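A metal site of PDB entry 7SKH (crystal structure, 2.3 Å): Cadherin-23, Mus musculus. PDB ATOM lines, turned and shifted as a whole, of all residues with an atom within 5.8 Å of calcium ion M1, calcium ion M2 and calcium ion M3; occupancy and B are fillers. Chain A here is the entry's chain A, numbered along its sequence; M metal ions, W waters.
Six residues have an atom within 4 Å of calcium ion M3: Asn 110, Asn 112, Asp 142, Asp 144, Asn 148 and Asp 197.
Water W2 bridges the side-chain amide nitrogen (ND2) of Asn 112 (3.1 Å) and the guanidinium group (NH1) of Arg 143 (3.3 Å).
Of the 21 residues printed, 4 come within 4 Å of calcium ion M2.
The nearest printed residue that does not touch calcium ion M2 is Tyr 72 (4.2 Å).
Calcium ion M1 is bound by OD1 of Asp 108 (2.3 Å), OD1 of Asp 111 (2.3 Å), OE1 of Glu 17 (2.3 Å), OE2 of Glu 73 (2.4 Å), O of Ile 109 (2.4 Å), OD1 of Asp 144 (2.5 Å) and OE1 of Glu 73 (2.7 Å).
Calcium ion M1 has seven donor atoms within binding distance.
Seven residues have an atom within 4 Å of calcium ion M1: Glu 17, Glu 73, Asp 108, Ile 109, Asp 111, Asn 112 and Asp 144.
Along chain A the residues within 4 Å of calcium ion M1 span positions 17 to 144.
The nearest printed residue that does not touch calcium ion M1 is Tyr 72 (4.5 Å).
Calcium ion M2 is bound by OE1 of Glu 73 (2.2 Å), OD1 of Asp 71 (2.2 Å), OE2 of Glu 17 (2.3 Å), OD2 of Asp 111 (2.3 Å), water W2 (2.4 Å) and water W1 (2.6 Å).
Calcium ion M2 has six donor atoms within binding distance.
Calcium ion M3 is bound by O of Asn 112, OD2 of Asp 144, OD1 of Asn 110, O of Asn 148, OD2 of Asp 197, OD2 of Asp 142 and OD1 of Asp 142.
OD2 of Asp 108 is in hydrogen-bond range of N of Ser 145.
OD1 of Asp 111 sits close to ND2 of Asn 112, at 3.1 Å.
The side-chain carboxylate of Glu 17 sits close to the backbone NH of Tyr 72.
The backbone NH of Asp 197 lies within hydrogen-bond range of the backbone carbonyl oxygen of Leu 203 (2.9 Å).
The side-chain amide oxygen (OD1) of Asn 112 sits at hydrogen-bond distance from the guanidinium group (NH1) of Arg 143, 2.7 Å away.
The side-chain carboxylate of Glu 73 sits close to the side-chain amide nitrogen of Asn 112, 3.2 Å away.
OD2 of Asp 108 is in hydrogen-bond range of ND2 of Asn 148 (3.4 Å).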
ATOM      1  N   GLU A  17     -32.306   0.985 -15.323  1.00  0.00           N
ATOM      2  CA  GLU A  17     -32.885   1.299 -16.639  1.00  0.00           C
ATOM      3  C   GLU A  17     -34.157   0.459 -16.809  1.00  0.00           C
ATOM      4  O   GLU A  17     -34.368  -0.459 -16.015  1.00  0.00           O
ATOM      5  CB  GLU A  17     -31.894   0.983 -17.751  1.00  0.00           C
ATOM      6  CG  GLU A  17     -31.740  -0.503 -18.003  1.00  0.00           C
ATOM      7  CD  GLU A  17     -30.970  -0.800 -19.270  1.00  0.00           C
ATOM      8  OE1 GLU A  17     -30.226  -1.831 -19.291  1.00  0.00           O
ATOM      9  OE2 GLU A  17     -31.121  -0.010 -20.254  1.00  0.00           O
ATOM     10  N   GLU A  69     -37.769   6.292 -21.676  1.00  0.00           N
ATOM     11  CA  GLU A  69     -37.170   5.181 -20.922  1.00  0.00           C
ATOM     12  C   GLU A  69     -35.693   5.500 -20.623  1.00  0.00           C
ATOM     13  O   GLU A  69     -34.946   5.883 -21.525  1.00  0.00           O
ATOM     14  CB  GLU A  69     -37.380   3.932 -21.768  1.00  0.00           C
ATOM     15  CG  GLU A  69     -36.985   2.688 -21.050  1.00  0.00           C
ATOM     16  CD  GLU A  69     -37.082   1.471 -21.927  1.00  0.00           C
ATOM     17  OE1 GLU A  69     -37.908   1.513 -22.838  1.00  0.00           O
ATOM     18  OE2 GLU A  69     -36.314   0.507 -21.687  1.00  0.00           O
ATOM     19  N   LEU A  70     -35.290   5.384 -19.368  1.00  0.00           N
ATOM     20  CA  LEU A  70     -33.860   5.404 -18.990  1.00  0.00           C
ATOM     21  C   LEU A  70     -33.237   4.171 -19.594  1.00  0.00           C
ATOM     22  O   LEU A  70     -33.835   3.095 -19.494  1.00  0.00           O
ATOM     23  CB  LEU A  70     -33.756   5.396 -17.475  1.00  0.00           C
ATOM     24  CG  LEU A  70     -34.262   6.659 -16.781  1.00  0.00           C
ATOM     25  CD1 LEU A  70     -33.691   6.756 -15.379  1.00  0.00           C
ATOM     26  CD2 LEU A  70     -33.886   7.896 -17.583  1.00  0.00           C
ATOM     27  N   ASP A  71     -32.096   4.325 -20.207  1.00  0.00           N
ATOM     28  CA  ASP A  71     -31.484   3.292 -21.071  1.00  0.00           C
ATOM     29  C   ASP A  71     -29.992   3.309 -20.771  1.00  0.00           C
ATOM     30  O   ASP A  71     -29.328   4.327 -21.058  1.00  0.00           O
ATOM     31  CB  ASP A  71     -31.743   3.560 -22.551  1.00  0.00           C
ATOM     32  CG  ASP A  71     -31.174   2.492 -23.476  1.00  0.00           C
ATOM     33  OD1 ASP A  71     -30.864   1.374 -22.966  1.00  0.00           O
ATOM     34  OD2 ASP A  71     -31.020   2.769 -24.673  1.00  0.00           O
ATOM     35  N   TYR A  72     -29.497   2.211 -20.205  1.00  0.00           N
ATOM     36  CA  TYR A  72     -28.052   2.032 -19.961  1.00  0.00           C
ATOM     37  C   TYR A  72     -27.303   2.094 -21.287  1.00  0.00           C
ATOM     38  O   TYR A  72     -26.180   2.564 -21.278  1.00  0.00           O
ATOM     39  CB  TYR A  72     -27.786   0.715 -19.237  1.00  0.00           C
ATOM     40  CG  TYR A  72     -26.364   0.588 -18.754  1.00  0.00           C
ATOM     41  CD1 TYR A  72     -25.388   0.110 -19.597  1.00  0.00           C
ATOM     42  CD2 TYR A  72     -26.004   0.944 -17.463  1.00  0.00           C
ATOM     43  CE1 TYR A  72     -24.080  -0.040 -19.163  1.00  0.00           C
ATOM     44  CE2 TYR A  72     -24.697   0.834 -17.019  1.00  0.00           C
ATOM     45  CZ  TYR A  72     -23.738   0.326 -17.869  1.00  0.00           C
ATOM     46  OH  TYR A  72     -22.428   0.182 -17.493  1.00  0.00           O
ATOM     47  N   GLU A  73     -27.889   1.595 -22.379  1.00  0.00           N
ATOM     48  CA  GLU A  73     -27.148   1.440 -23.645  1.00  0.00           C
ATOM     49  C   GLU A  73     -26.946   2.808 -24.299  1.00  0.00           C
ATOM     50  O   GLU A  73     -26.010   2.942 -25.061  1.00  0.00           O
ATOM     51  CB  GLU A  73     -27.845   0.439 -24.570  1.00  0.00           C
ATOM     52  CG  GLU A  73     -27.631  -1.013 -24.175  1.00  0.00           C
ATOM     53  CD  GLU A  73     -28.213  -1.484 -22.840  1.00  0.00           C
ATOM     54  OE1 GLU A  73     -29.398  -1.358 -22.621  1.00  0.00           O
ATOM     55  OE2 GLU A  73     -27.479  -2.055 -22.029  1.00  0.00           O
ATOM     56  N   ASP A 108     -27.397  -1.386 -15.499  1.00  0.00           N
ATOM     57  CA  ASP A 108     -27.630  -2.252 -16.679  1.00  0.00           C
ATOM     58  C   ASP A 108     -28.575  -3.404 -16.298  1.00  0.00           C
ATOM     59  O   ASP A 108     -28.338  -4.019 -15.291  1.00  0.00           O
ATOM     60  CB  ASP A 108     -26.310  -2.775 -17.217  1.00  0.00           C
ATOM     61  CG  ASP A 108     -26.405  -3.511 -18.547  1.00  0.00           C
ATOM     62  OD1 ASP A 108     -27.321  -3.202 -19.350  1.00  0.00           O
ATOM     63  OD2 ASP A 108     -25.536  -4.365 -18.784  1.00  0.00           O
ATOM     64  N   ILE A 109     -29.655  -3.624 -17.062  1.00  0.00           N
ATOM     65  CA  ILE A 109     -30.456  -4.894 -17.001  1.00  0.00           C
ATOM     66  C   ILE A 109     -30.271  -5.642 -18.335  1.00  0.00           C
ATOM     67  O   ILE A 109     -29.917  -5.012 -19.363  1.00  0.00           O
ATOM     68  CB  ILE A 109     -31.949  -4.634 -16.671  1.00  0.00           C
ATOM     69  CG1 ILE A 109     -32.753  -4.104 -17.855  1.00  0.00           C
ATOM     70  CG2 ILE A 109     -32.086  -3.724 -15.450  1.00  0.00           C
ATOM     71  CD1 ILE A 109     -34.254  -3.884 -17.566  1.00  0.00           C
ATOM     72  N   ASN A 110     -30.552  -6.934 -18.313  1.00  0.00           N
ATOM     73  CA  ASN A 110     -30.411  -7.812 -19.488  1.00  0.00           C
ATOM     74  C   ASN A 110     -31.640  -7.581 -20.380  1.00  0.00           C
ATOM     75  O   ASN A 110     -32.600  -8.377 -20.284  1.00  0.00           O
ATOM     76  CB  ASN A 110     -30.206  -9.265 -19.078  1.00  0.00           C
ATOM     77  CG  ASN A 110     -29.667 -10.073 -20.229  1.00  0.00           C
ATOM     78  OD1 ASN A 110     -28.923  -9.550 -21.062  1.00  0.00           O
ATOM     79  ND2 ASN A 110     -29.979 -11.362 -20.252  1.00  0.00           N
ATOM     80  N   ASP A 111     -31.613  -6.523 -21.192  1.00  0.00           N
ATOM     81  CA  ASP A 111     -32.719  -6.173 -22.125  1.00  0.00           C
ATOM     82  C   ASP A 111     -32.247  -6.251 -23.591  1.00  0.00           C
ATOM     83  O   ASP A 111     -33.004  -5.772 -24.442  1.00  0.00           O
ATOM     84  CB  ASP A 111     -33.343  -4.805 -21.787  1.00  0.00           C
ATOM     85  CG  ASP A 111     -32.382  -3.614 -21.773  1.00  0.00           C
ATOM     86  OD1 ASP A 111     -31.140  -3.831 -21.785  1.00  0.00           O
ATOM     87  OD2 ASP A 111     -32.877  -2.478 -21.759  1.00  0.00           O
ATOM     88  N   ASN A 112     -31.062  -6.799 -23.901  1.00  0.00           N
ATOM     89  CA  ASN A 112     -30.591  -6.997 -25.296  1.00  0.00           C
ATOM     90  C   ASN A 112     -30.278  -8.489 -25.496  1.00  0.00           C
ATOM     91  O   ASN A 112     -29.560  -9.084 -24.649  1.00  0.00           O
ATOM     92  CB  ASN A 112     -29.440  -6.052 -25.658  1.00  0.00           C
ATOM     93  CG  ASN A 112     -29.907  -4.604 -25.686  1.00  0.00           C
ATOM     94  OD1 ASN A 112     -30.409  -4.142 -26.698  1.00  0.00           O
ATOM     95  ND2 ASN A 112     -29.811  -3.910 -24.566  1.00  0.00           N
ATOM     96  N   VAL A 113     -30.871  -9.068 -26.537  1.00  0.00           N
ATOM     97  CA  VAL A 113     -30.683 -10.478 -26.972  1.00  0.00           C
ATOM     98  C   VAL A 113     -29.360 -10.551 -27.731  1.00  0.00           C
ATOM     99  O   VAL A 113     -29.088  -9.665 -28.539  1.00  0.00           O
ATOM    100  CB  VAL A 113     -31.849 -10.909 -27.882  1.00  0.00           C
ATOM    101  CG1 VAL A 113     -31.753 -12.375 -28.242  1.00  0.00           C
ATOM    102  CG2 VAL A 113     -33.214 -10.609 -27.280  1.00  0.00           C
ATOM    103  N   PRO A 114     -28.502 -11.569 -27.476  1.00  0.00           N
ATOM    104  CA  PRO A 114     -27.294 -11.756 -28.276  1.00  0.00           C
ATOM    105  C   PRO A 114     -27.770 -12.086 -29.687  1.00  0.00           C
ATOM    106  O   PRO A 114     -28.502 -13.035 -29.810  1.00  0.00           O
ATOM    107  CB  PRO A 114     -26.561 -12.933 -27.644  1.00  0.00           C
ATOM    108  CG  PRO A 114     -27.572 -13.593 -26.709  1.00  0.00           C
ATOM    109  CD  PRO A 114     -28.646 -12.581 -26.420  1.00  0.00           C
ATOM    110  N   ASP A 142     -23.983  -8.547 -28.400  1.00  0.00           N
ATOM    111  CA  ASP A 142     -24.907  -8.242 -27.276  1.00  0.00           C
ATOM    112  C   ASP A 142     -24.639  -6.808 -26.813  1.00  0.00           C
ATOM    113  O   ASP A 142     -23.563  -6.548 -26.317  1.00  0.00           O
ATOM    114  CB  ASP A 142     -24.754  -9.297 -26.177  1.00  0.00           C
ATOM    115  CG  ASP A 142     -25.909  -9.278 -25.210  1.00  0.00           C
ATOM    116  OD1 ASP A 142     -26.221  -8.181 -24.696  1.00  0.00           O
ATOM    117  OD2 ASP A 142     -26.485 -10.346 -24.976  1.00  0.00           O
ATOM    118  N   ARG A 143     -25.631  -5.939 -26.902  1.00  0.00           N
ATOM    119  CA  ARG A 143     -25.496  -4.481 -26.630  1.00  0.00           C
ATOM    120  C   ARG A 143     -25.341  -4.232 -25.125  1.00  0.00           C
ATOM    121  O   ARG A 143     -24.940  -3.133 -24.776  1.00  0.00           O
ATOM    122  CB  ARG A 143     -26.717  -3.722 -27.177  1.00  0.00           C
ATOM    123  CG  ARG A 143     -26.667  -3.466 -28.685  1.00  0.00           C
ATOM    124  CD  ARG A 143     -27.990  -2.942 -29.242  1.00  0.00           C
ATOM    125  NE  ARG A 143     -28.154  -1.498 -29.038  1.00  0.00           N
ATOM    126  CZ  ARG A 143     -28.936  -0.940 -28.128  1.00  0.00           C
ATOM    127  NH1 ARG A 143     -29.681  -1.670 -27.331  1.00  0.00           N
ATOM    128  NH2 ARG A 143     -28.978   0.367 -28.030  1.00  0.00           N
ATOM    129  N   ASP A 144     -25.694  -5.205 -24.270  1.00  0.00           N
ATOM    130  CA  ASP A 144     -25.537  -5.052 -22.792  1.00  0.00           C
ATOM    131  C   ASP A 144     -24.066  -5.090 -22.401  1.00  0.00           C
ATOM    132  O   ASP A 144     -23.215  -5.343 -23.255  1.00  0.00           O
ATOM    133  CB  ASP A 144     -26.325  -6.124 -22.005  1.00  0.00           C
ATOM    134  CG  ASP A 144     -27.806  -6.149 -22.339  1.00  0.00           C
ATOM    135  OD1 ASP A 144     -28.427  -5.095 -22.284  1.00  0.00           O
ATOM    136  OD2 ASP A 144     -28.308  -7.220 -22.691  1.00  0.00           O
ATOM    137  N   SER A 145     -23.794  -4.781 -21.139  1.00  0.00           N
ATOM    138  CA  SER A 145     -22.457  -4.758 -20.514  1.00  0.00           C
ATOM    139  C   SER A 145     -22.357  -5.826 -19.413  1.00  0.00           C
ATOM    140  O   SER A 145     -23.375  -6.445 -19.069  1.00  0.00           O
ATOM    141  CB  SER A 145     -22.167  -3.379 -19.974  1.00  0.00           C
ATOM    142  OG  SER A 145     -22.080  -2.488 -21.059  1.00  0.00           O
ATOM    143  N   ASN A 148     -24.280  -9.564 -18.634  1.00  0.00           N
ATOM    144  CA  ASN A 148     -25.484  -9.319 -19.451  1.00  0.00           C
ATOM    145  C   ASN A 148     -25.061  -9.270 -20.915  1.00  0.00           C
ATOM    146  O   ASN A 148     -25.859  -9.576 -21.762  1.00  0.00           O
ATOM    147  CB  ASN A 148     -26.178  -8.023 -19.052  1.00  0.00           C
ATOM    148  CG  ASN A 148     -26.890  -8.045 -17.707  1.00  0.00           C
ATOM    149  OD1 ASN A 148     -27.300  -9.082 -17.212  1.00  0.00           O
ATOM    150  ND2 ASN A 148     -27.116  -6.858 -17.176  1.00  0.00           N
ATOM    151  N   GLY A 149     -23.831  -8.849 -21.189  1.00  0.00           N
ATOM    152  CA  GLY A 149     -23.292  -8.714 -22.547  1.00  0.00           C
ATOM    153  C   GLY A 149     -22.368  -9.822 -22.971  1.00  0.00           C
ATOM    154  O   GLY A 149     -21.872  -9.730 -24.108  1.00  0.00           O
ATOM    155  N   ASP A 197     -26.481 -15.293 -23.503  1.00  0.00           N
ATOM    156  CA  ASP A 197     -25.729 -14.328 -22.656  1.00  0.00           C
ATOM    157  C   ASP A 197     -25.690 -14.862 -21.230  1.00  0.00           C
ATOM    158  O   ASP A 197     -26.278 -15.899 -20.967  1.00  0.00           O
ATOM    159  CB  ASP A 197     -26.269 -12.916 -22.823  1.00  0.00           C
ATOM    160  CG  ASP A 197     -27.662 -12.723 -22.298  1.00  0.00           C
ATOM    161  OD1 ASP A 197     -28.056 -13.489 -21.392  1.00  0.00           O
ATOM    162  OD2 ASP A 197     -28.324 -11.791 -22.759  1.00  0.00           O
ATOM    163  N   LEU A 203     -30.805 -14.398 -22.085  1.00  0.00           N
ATOM    164  CA  LEU A 203     -31.450 -14.251 -23.412  1.00  0.00           C
ATOM    165  C   LEU A 203     -30.563 -14.983 -24.421  1.00  0.00           C
ATOM    166  O   LEU A 203     -29.300 -14.982 -24.229  1.00  0.00           O
ATOM    167  CB  LEU A 203     -31.631 -12.779 -23.760  1.00  0.00           C
ATOM    168  CG  LEU A 203     -32.544 -11.948 -22.839  1.00  0.00           C
ATOM    169  CD1 LEU A 203     -32.384 -10.468 -23.120  1.00  0.00           C
ATOM    170  CD2 LEU A 203     -34.008 -12.363 -22.957  1.00  0.00           C
HETATM  171 CA    CA M   1     -29.109  -3.257 -20.786  1.00  0.00          CA
HETATM  172 CA    CA M   2     -31.525  -0.699 -22.406  1.00  0.00          CA
HETATM  173 CA    CA M   3     -27.832  -9.463 -23.133  1.00  0.00          CA
HETATM  174  O   HOH W   1     -33.713   0.634 -22.445  1.00  0.00           O
HETATM  175  O   HOH W   2     -31.623  -1.455 -24.678  1.00  0.00           O
